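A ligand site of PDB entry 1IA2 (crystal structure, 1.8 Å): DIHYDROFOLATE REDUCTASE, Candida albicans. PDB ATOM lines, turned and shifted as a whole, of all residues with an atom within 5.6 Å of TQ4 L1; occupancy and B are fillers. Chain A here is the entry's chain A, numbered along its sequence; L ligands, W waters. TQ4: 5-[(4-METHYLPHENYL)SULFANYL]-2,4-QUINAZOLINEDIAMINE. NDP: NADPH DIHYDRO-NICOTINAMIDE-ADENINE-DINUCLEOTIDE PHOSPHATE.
OE1 of Glu 32 lies within hydrogen-bond range of N6 of TQ4 L1 (2.6 Å).
The backbone carbonyl oxygen of Ile 9 sits at hydrogen-bond distance from a nitrogen (N7) of TQ4 L1 (3.0 Å).
The backbone carbonyl oxygen of Ile 112 is in hydrogen-bond range of a nitrogen (N7) of TQ4 L1 (3.0 Å).
N7 of TQ4 L1 lies within hydrogen-bond range of OH of Tyr 118.
An oxygen (O7N) of NDP L2 lies within hydrogen-bond range of the backbone NH (N) of Ala 11, at 2.9 Å.
O of Ala 11 lies within hydrogen-bond range of N7N of NDP L2.
The backbone NH (N) of Thr 58 is in hydrogen-bond range of an oxygen (O2A) of NDP L2 (3.1 Å).
The side-chain hydroxyl (OG1) of Thr 58 is in hydrogen-bond range of an oxygen (O2A) of NDP L2.
The backbone NH of Met 25 sits at hydrogen-bond distance from an oxygen (O2D) of NDP L2 (3.4 Å).
The side-chain carboxylate of Glu 32 is in hydrogen-bond range of the side-chain hydroxyl of Thr 133, 2.5 Å away.
The backbone carbonyl oxygen (O) of Ile 9 lies within hydrogen-bond range of the side-chain hydroxyl (OH) of Tyr 118 (2.8 Å).
The backbone NH of Ile 9 sits at hydrogen-bond distance from the backbone carbonyl oxygen of Ile 111.
The backbone carbonyl oxygen (O) of Ile 112 sits at hydrogen-bond distance from the side-chain hydroxyl (OH) of Tyr 118 (3.0 Å).
The backbone NH (N) of Thr 133 sits at hydrogen-bond distance from the backbone carbonyl oxygen (O) of Val 10, 2.8 Å away.
N of Val 10 sits at hydrogen-bond distance from O of Leu 131 (3.0 Å).
Residues that only touch TQ4 L1: Val 10 (3.4 Å), Ala 11 (3.7 Å), Ile 33 (3.5 Å), Phe 36 (3.4 Å), Thr 58 (3.8 Å), Ser 61 (3.7 Å), Ile 62 (3.9 Å) and Thr 133 (3.7 Å).
Hydrophobic or aromatic side chains that line TQ4 L1: Ile 9, Ala 11, Ile 33, Phe 36, Ile 62 and Ile 112.
The nearest printed residue that does not touch TQ4 L1 is Met 25 (4.1 Å).
Water W2 lies within hydrogen-bond range of OG1 of Thr 133, O of Leu 131, N14 of TQ4 L1 and O of Val 10.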
ATOM      1  N   ILE A   9       3.615  18.587 -33.950  1.00  0.00           N
ATOM      2  CA  ILE A   9       2.808  19.857 -34.145  1.00  0.00           C
ATOM      3  C   ILE A   9       2.228  20.176 -32.764  1.00  0.00           C
ATOM      4  O   ILE A   9       1.641  19.296 -32.113  1.00  0.00           O
ATOM      5  CB  ILE A   9       1.740  19.694 -35.270  1.00  0.00           C
ATOM      6  CG1 ILE A   9       0.945  21.061 -35.379  1.00  0.00           C
ATOM      7  CG2 ILE A   9       0.781  18.527 -35.028  1.00  0.00           C
ATOM      8  CD1 ILE A   9       0.110  21.203 -36.659  1.00  0.00           C
ATOM      9  N   VAL A  10       2.460  21.417 -32.320  1.00  0.00           N
ATOM     10  CA  VAL A  10       2.024  21.845 -30.952  1.00  0.00           C
ATOM     11  C   VAL A  10       1.772  23.341 -30.925  1.00  0.00           C
ATOM     12  O   VAL A  10       2.416  24.093 -31.704  1.00  0.00           O
ATOM     13  CB  VAL A  10       3.162  21.451 -29.957  1.00  0.00           C
ATOM     14  CG1 VAL A  10       4.482  22.109 -30.311  1.00  0.00           C
ATOM     15  CG2 VAL A  10       2.797  21.705 -28.492  1.00  0.00           C
ATOM     16  N   ALA A  11       1.002  23.806 -29.965  1.00  0.00           N
ATOM     17  CA  ALA A  11       0.762  25.232 -29.742  1.00  0.00           C
ATOM     18  C   ALA A  11       1.297  25.557 -28.349  1.00  0.00           C
ATOM     19  O   ALA A  11       0.925  24.838 -27.390  1.00  0.00           O
ATOM     20  CB  ALA A  11      -0.719  25.563 -29.867  1.00  0.00           C
ATOM     21  N   MET A  25      -6.045  22.427 -22.580  1.00  0.00           N
ATOM     22  CA  MET A  25      -5.334  23.599 -23.143  1.00  0.00           C
ATOM     23  C   MET A  25      -5.932  24.808 -22.426  1.00  0.00           C
ATOM     24  O   MET A  25      -7.154  24.869 -22.231  1.00  0.00           O
ATOM     25  CB  MET A  25      -5.442  23.651 -24.674  1.00  0.00           C
ATOM     26  CG  MET A  25      -4.756  22.449 -25.265  1.00  0.00           C
ATOM     27  SD  MET A  25      -5.062  22.307 -27.058  1.00  0.00           S
ATOM     28  CE  MET A  25      -4.062  23.688 -27.666  1.00  0.00           C
ATOM     29  N   GLU A  32      -6.608  28.701 -34.786  1.00  0.00           N
ATOM     30  CA  GLU A  32      -5.456  27.737 -34.575  1.00  0.00           C
ATOM     31  C   GLU A  32      -5.938  26.338 -34.744  1.00  0.00           C
ATOM     32  O   GLU A  32      -5.200  25.535 -35.365  1.00  0.00           O
ATOM     33  CB  GLU A  32      -4.798  27.954 -33.219  1.00  0.00           C
ATOM     34  CG  GLU A  32      -3.267  27.680 -33.126  1.00  0.00           C
ATOM     35  CD  GLU A  32      -2.952  26.204 -33.086  1.00  0.00           C
ATOM     36  OE1 GLU A  32      -3.709  25.402 -32.569  1.00  0.00           O
ATOM     37  OE2 GLU A  32      -1.910  25.864 -33.662  1.00  0.00           O
ATOM     38  N   ILE A  33      -7.099  25.972 -34.187  1.00  0.00           N
ATOM     39  CA  ILE A  33      -7.650  24.625 -34.352  1.00  0.00           C
ATOM     40  C   ILE A  33      -7.870  24.313 -35.842  1.00  0.00           C
ATOM     41  O   ILE A  33      -7.676  23.202 -36.311  1.00  0.00           O
ATOM     42  CB  ILE A  33      -9.006  24.423 -33.568  1.00  0.00           C
ATOM     43  CG1 ILE A  33      -8.945  24.917 -32.138  1.00  0.00           C
ATOM     44  CG2 ILE A  33      -9.534  22.963 -33.745  1.00  0.00           C
ATOM     45  CD1 ILE A  33      -7.983  24.327 -31.139  1.00  0.00           C
ATOM     46  N   TYR A  35      -6.263  25.512 -38.377  1.00  0.00           N
ATOM     47  CA  TYR A  35      -4.921  25.333 -38.984  1.00  0.00           C
ATOM     48  C   TYR A  35      -4.440  23.867 -38.696  1.00  0.00           C
ATOM     49  O   TYR A  35      -3.976  23.205 -39.619  1.00  0.00           O
ATOM     50  CB  TYR A  35      -3.884  26.270 -38.352  1.00  0.00           C
ATOM     51  CG  TYR A  35      -2.418  26.009 -38.600  1.00  0.00           C
ATOM     52  CD1 TYR A  35      -1.552  25.355 -37.709  1.00  0.00           C
ATOM     53  CD2 TYR A  35      -1.886  26.434 -39.811  1.00  0.00           C
ATOM     54  CE1 TYR A  35      -0.194  25.177 -38.032  1.00  0.00           C
ATOM     55  CE2 TYR A  35      -0.549  26.277 -40.147  1.00  0.00           C
ATOM     56  CZ  TYR A  35       0.284  25.628 -39.237  1.00  0.00           C
ATOM     57  OH  TYR A  35       1.610  25.537 -39.658  1.00  0.00           O
ATOM     58  N   PHE A  36      -4.569  23.545 -37.428  1.00  0.00           N
ATOM     59  CA  PHE A  36      -4.217  22.095 -37.066  1.00  0.00           C
ATOM     60  C   PHE A  36      -4.939  21.126 -37.942  1.00  0.00           C
ATOM     61  O   PHE A  36      -4.317  20.214 -38.527  1.00  0.00           O
ATOM     62  CB  PHE A  36      -4.337  21.922 -35.578  1.00  0.00           C
ATOM     63  CG  PHE A  36      -4.339  20.510 -35.090  1.00  0.00           C
ATOM     64  CD1 PHE A  36      -5.531  19.799 -34.992  1.00  0.00           C
ATOM     65  CD2 PHE A  36      -3.103  19.863 -34.858  1.00  0.00           C
ATOM     66  CE1 PHE A  36      -5.552  18.474 -34.529  1.00  0.00           C
ATOM     67  CE2 PHE A  36      -3.149  18.538 -34.394  1.00  0.00           C
ATOM     68  CZ  PHE A  36      -4.321  17.836 -34.267  1.00  0.00           C
ATOM     69  N   THR A  58      -4.232  11.530 -24.090  1.00  0.00           N
ATOM     70  CA  THR A  58      -4.831  12.488 -25.056  1.00  0.00           C
ATOM     71  C   THR A  58      -5.990  11.853 -25.788  1.00  0.00           C
ATOM     72  O   THR A  58      -7.053  12.481 -25.886  1.00  0.00           O
ATOM     73  CB  THR A  58      -3.758  13.125 -25.980  1.00  0.00           C
ATOM     74  OG1 THR A  58      -2.934  13.948 -25.119  1.00  0.00           O
ATOM     75  CG2 THR A  58      -4.318  13.940 -27.177  1.00  0.00           C
ATOM     76  N   SER A  61      -8.951  11.833 -23.748  1.00  0.00           N
ATOM     77  CA  SER A  61      -9.508  13.160 -23.556  1.00  0.00           C
ATOM     78  C   SER A  61     -10.441  13.595 -24.658  1.00  0.00           C
ATOM     79  O   SER A  61     -11.118  14.643 -24.555  1.00  0.00           O
ATOM     80  CB  SER A  61      -8.363  14.190 -23.382  1.00  0.00           C
ATOM     81  OG  SER A  61      -7.884  14.024 -22.042  1.00  0.00           O
ATOM     82  N   ILE A  62     -10.470  12.854 -25.739  1.00  0.00           N
ATOM     83  CA  ILE A  62     -11.396  13.263 -26.855  1.00  0.00           C
ATOM     84  C   ILE A  62     -12.701  12.526 -26.479  1.00  0.00           C
ATOM     85  O   ILE A  62     -12.664  11.323 -26.191  1.00  0.00           O
ATOM     86  CB  ILE A  62     -10.915  12.634 -28.221  1.00  0.00           C
ATOM     87  CG1 ILE A  62      -9.467  13.142 -28.512  1.00  0.00           C
ATOM     88  CG2 ILE A  62     -11.922  13.077 -29.334  1.00  0.00           C
ATOM     89  CD1 ILE A  62      -8.790  12.407 -29.694  1.00  0.00           C
ATOM     90  N   LEU A  69     -10.046  10.901 -34.860  1.00  0.00           N
ATOM     91  CA  LEU A  69     -10.050  12.173 -35.668  1.00  0.00           C
ATOM     92  C   LEU A  69     -10.252  11.754 -37.096  1.00  0.00           C
ATOM     93  O   LEU A  69      -9.638  10.836 -37.684  1.00  0.00           O
ATOM     94  CB  LEU A  69      -8.735  12.887 -35.336  1.00  0.00           C
ATOM     95  CG  LEU A  69      -8.419  13.320 -33.949  1.00  0.00           C
ATOM     96  CD1 LEU A  69      -7.037  13.994 -33.857  1.00  0.00           C
ATOM     97  CD2 LEU A  69      -9.460  14.223 -33.280  1.00  0.00           C
ATOM     98  N   ILE A 111       3.113  13.977 -34.828  1.00  0.00           N
ATOM     99  CA  ILE A 111       2.892  13.613 -33.349  1.00  0.00           C
ATOM    100  C   ILE A 111       2.087  14.805 -32.819  1.00  0.00           C
ATOM    101  O   ILE A 111       2.565  15.931 -32.955  1.00  0.00           O
ATOM    102  CB  ILE A 111       4.274  13.552 -32.597  1.00  0.00           C
ATOM    103  CG1 ILE A 111       5.082  12.334 -33.198  1.00  0.00           C
ATOM    104  CG2 ILE A 111       4.157  13.468 -31.092  1.00  0.00           C
ATOM    105  CD1 ILE A 111       6.602  12.406 -32.777  1.00  0.00           C
ATOM    106  N   ILE A 112       0.906  14.461 -32.275  1.00  0.00           N
ATOM    107  CA  ILE A 112       0.020  15.534 -31.803  1.00  0.00           C
ATOM    108  C   ILE A 112      -0.067  15.774 -30.313  1.00  0.00           C
ATOM    109  O   ILE A 112      -0.871  16.667 -29.981  1.00  0.00           O
ATOM    110  CB  ILE A 112      -1.381  15.438 -32.545  1.00  0.00           C
ATOM    111  CG1 ILE A 112      -2.143  14.193 -31.990  1.00  0.00           C
ATOM    112  CG2 ILE A 112      -1.140  15.413 -34.085  1.00  0.00           C
ATOM    113  CD1 ILE A 112      -3.659  14.163 -32.428  1.00  0.00           C
ATOM    114  N   GLY A 113       0.699  15.053 -29.507  1.00  0.00           N
ATOM    115  CA  GLY A 113       0.669  15.273 -28.044  1.00  0.00           C
ATOM    116  C   GLY A 113       0.393  13.952 -27.361  1.00  0.00           C
ATOM    117  O   GLY A 113       0.233  12.920 -27.924  1.00  0.00           O
ATOM    118  N   TYR A 118       5.518  14.282 -26.326  1.00  0.00           N
ATOM    119  CA  TYR A 118       6.341  15.336 -26.873  1.00  0.00           C
ATOM    120  C   TYR A 118       7.768  15.335 -26.290  1.00  0.00           C
ATOM    121  O   TYR A 118       8.745  15.336 -26.992  1.00  0.00           O
ATOM    122  CB  TYR A 118       5.718  16.728 -26.556  1.00  0.00           C
ATOM    123  CG  TYR A 118       4.513  17.137 -27.373  1.00  0.00           C
ATOM    124  CD1 TYR A 118       4.402  16.973 -28.765  1.00  0.00           C
ATOM    125  CD2 TYR A 118       3.550  17.895 -26.720  1.00  0.00           C
ATOM    126  CE1 TYR A 118       3.294  17.454 -29.454  1.00  0.00           C
ATOM    127  CE2 TYR A 118       2.422  18.383 -27.397  1.00  0.00           C
ATOM    128  CZ  TYR A 118       2.311  18.184 -28.727  1.00  0.00           C
ATOM    129  OH  TYR A 118       1.240  18.683 -29.413  1.00  0.00           O
ATOM    130  N   LEU A 131       6.477  21.927 -35.962  1.00  0.00           N
ATOM    131  CA  LEU A 131       5.543  23.051 -36.319  1.00  0.00           C
ATOM    132  C   LEU A 131       5.019  23.517 -34.930  1.00  0.00           C
ATOM    133  O   LEU A 131       4.178  22.855 -34.376  1.00  0.00           O
ATOM    134  CB  LEU A 131       4.400  22.421 -37.145  1.00  0.00           C
ATOM    135  CG  LEU A 131       4.735  21.841 -38.484  1.00  0.00           C
ATOM    136  CD1 LEU A 131       3.598  20.928 -38.966  1.00  0.00           C
ATOM    137  CD2 LEU A 131       4.935  22.978 -39.487  1.00  0.00           C
ATOM    138  N   THR A 133       3.202  26.505 -32.890  1.00  0.00           N
ATOM    139  CA  THR A 133       2.426  27.851 -32.986  1.00  0.00           C
ATOM    140  C   THR A 133       2.938  28.577 -31.768  1.00  0.00           C
ATOM    141  O   THR A 133       2.621  28.070 -30.659  1.00  0.00           O
ATOM    142  CB  THR A 133       0.903  27.573 -32.916  1.00  0.00           C
ATOM    143  OG1 THR A 133       0.415  26.778 -34.010  1.00  0.00           O
ATOM    144  CG2 THR A 133       0.092  28.903 -32.803  1.00  0.00           C
HETATM  145  C1  TQ4 L   1      -3.812  21.980 -31.723  1.00  0.00           C
HETATM  146  C2  TQ4 L   1      -3.368  20.684 -31.405  1.00  0.00           C
HETATM  147  C3  TQ4 L   1      -1.923  20.419 -31.729  1.00  0.00           C
HETATM  148  N4  TQ4 L   1      -1.156  21.278 -32.230  1.00  0.00           N
HETATM  149  C5  TQ4 L   1      -1.589  22.516 -32.588  1.00  0.00           C
HETATM  150  N6  TQ4 L   1      -2.901  22.923 -32.299  1.00  0.00           N
HETATM  151  N7  TQ4 L   1      -1.273  19.253 -31.500  1.00  0.00           N
HETATM  152  C8  TQ4 L   1      -5.141  22.381 -31.518  1.00  0.00           C
HETATM  153  C9  TQ4 L   1      -6.023  21.480 -30.959  1.00  0.00           C
HETATM  154  C12 TQ4 L   1      -5.621  20.173 -30.679  1.00  0.00           C
HETATM  155  C13 TQ4 L   1      -4.303  19.783 -30.903  1.00  0.00           C
HETATM  156  N14 TQ4 L   1      -0.821  23.403 -33.139  1.00  0.00           N
HETATM  157  S20 TQ4 L   1      -3.953  18.086 -30.572  1.00  0.00           S
HETATM  158  C22 TQ4 L   1      -5.172  17.581 -29.438  1.00  0.00           C
HETATM  159  C23 TQ4 L   1      -5.174  18.119 -28.155  1.00  0.00           C
HETATM  160  C24 TQ4 L   1      -6.121  17.657 -27.231  1.00  0.00           C
HETATM  161  C25 TQ4 L   1      -7.026  16.647 -27.548  1.00  0.00           C
HETATM  162  C26 TQ4 L   1      -6.967  16.085 -28.813  1.00  0.00           C
HETATM  163  C27 TQ4 L   1      -6.045  16.546 -29.770  1.00  0.00           C
HETATM  164  C32 TQ4 L   1      -8.025  16.142 -26.495  1.00  0.00           C
HETATM  165  PA  NDP L   2      -0.142  12.031 -23.187  1.00  0.00           P
HETATM  166  O1A NDP L   2       1.176  12.482 -23.381  1.00  0.00           O
HETATM  167  O2A NDP L   2      -1.200  12.333 -24.185  1.00  0.00           O
HETATM  168  O5B NDP L   2      -0.280  10.538 -22.689  1.00  0.00           O
HETATM  169  C5B NDP L   2       0.815   9.970 -21.878  1.00  0.00           C
HETATM  170  C4B NDP L   2       0.615   8.493 -21.920  1.00  0.00           C
HETATM  171  O4B NDP L   2       1.087   8.047 -23.258  1.00  0.00           O
HETATM  172  C3B NDP L   2       1.421   7.627 -20.904  1.00  0.00           C
HETATM  173  O3B NDP L   2       0.639   7.543 -19.690  1.00  0.00           O
HETATM  174  C2B NDP L   2       1.608   6.309 -21.714  1.00  0.00           C
HETATM  175  O2B NDP L   2       0.478   5.402 -21.861  1.00  0.00           O
HETATM  176  C1B NDP L   2       1.793   6.845 -23.098  1.00  0.00           C
HETATM  177  N9A NDP L   2       3.153   7.060 -23.438  1.00  0.00           N
HETATM  178  C8A NDP L   2       3.876   8.168 -23.075  1.00  0.00           C
HETATM  179  N7A NDP L   2       5.120   8.130 -23.564  1.00  0.00           N
HETATM  180  C5A NDP L   2       5.152   6.915 -24.196  1.00  0.00           C
HETATM  181  C6A NDP L   2       6.220   6.336 -24.903  1.00  0.00           C
HETATM  182  N6A NDP L   2       7.400   6.965 -24.959  1.00  0.00           N
HETATM  183  N1A NDP L   2       5.991   5.120 -25.439  1.00  0.00           N
HETATM  184  C2A NDP L   2       4.749   4.567 -25.326  1.00  0.00           C
HETATM  185  N3A NDP L   2       3.697   5.002 -24.706  1.00  0.00           N
HETATM  186  C4A NDP L   2       3.960   6.267 -24.176  1.00  0.00           C
HETATM  187  O3  NDP L   2      -0.592  12.805 -21.846  1.00  0.00           O
HETATM  188  PN  NDP L   2      -0.022  13.902 -20.883  1.00  0.00           P
HETATM  189  O1N NDP L   2      -0.885  13.873 -19.672  1.00  0.00           O
HETATM  190  O2N NDP L   2       1.425  13.850 -20.604  1.00  0.00           O
HETATM  191  O5D NDP L   2      -0.309  15.289 -21.660  1.00  0.00           O
HETATM  192  C5D NDP L   2      -1.621  15.891 -21.651  1.00  0.00           C
HETATM  193  C4D NDP L   2      -1.444  17.397 -21.626  1.00  0.00           C
HETATM  194  O4D NDP L   2      -0.860  17.878 -22.878  1.00  0.00           O
HETATM  195  C3D NDP L   2      -2.729  18.208 -21.412  1.00  0.00           C
HETATM  196  O3D NDP L   2      -2.516  19.339 -20.568  1.00  0.00           O
HETATM  197  C2D NDP L   2      -3.055  18.608 -22.872  1.00  0.00           C
HETATM  198  O2D NDP L   2      -3.890  19.762 -22.881  1.00  0.00           O
HETATM  199  C1D NDP L   2      -1.670  18.901 -23.428  1.00  0.00           C
HETATM  200  N1N NDP L   2      -1.648  18.913 -24.917  1.00  0.00           N
HETATM  201  C2N NDP L   2      -1.327  20.166 -25.467  1.00  0.00           C
HETATM  202  C3N NDP L   2      -1.288  20.320 -26.820  1.00  0.00           C
HETATM  203  C7N NDP L   2      -0.911  21.742 -27.367  1.00  0.00           C
HETATM  204  O7N NDP L   2      -0.747  21.955 -28.510  1.00  0.00           O
HETATM  205  N7N NDP L   2      -0.751  22.769 -26.427  1.00  0.00           N
HETATM  206  C4N NDP L   2      -1.551  19.246 -27.730  1.00  0.00           C
HETATM  207  C5N NDP L   2      -1.885  18.055 -27.065  1.00  0.00           C
HETATM  208  C6N NDP L   2      -1.934  17.828 -25.735  1.00  0.00           C
HETATM  209  P2B NDP L   2       0.318   4.277 -20.633  1.00  0.00           P
HETATM  210  O1X NDP L   2      -0.976   3.664 -21.030  1.00  0.00           O
HETATM  211  O2X NDP L   2       1.624   3.532 -20.882  1.00  0.00           O
HETATM  212  O3X NDP L   2       0.374   5.096 -19.444  1.00  0.00           O
HETATM  213  O   HOH W   1      -6.430  17.438 -23.756  1.00  0.00           O
HETATM  214  O   HOH W   2       1.802  24.530 -35.115  1.00  0.00           O
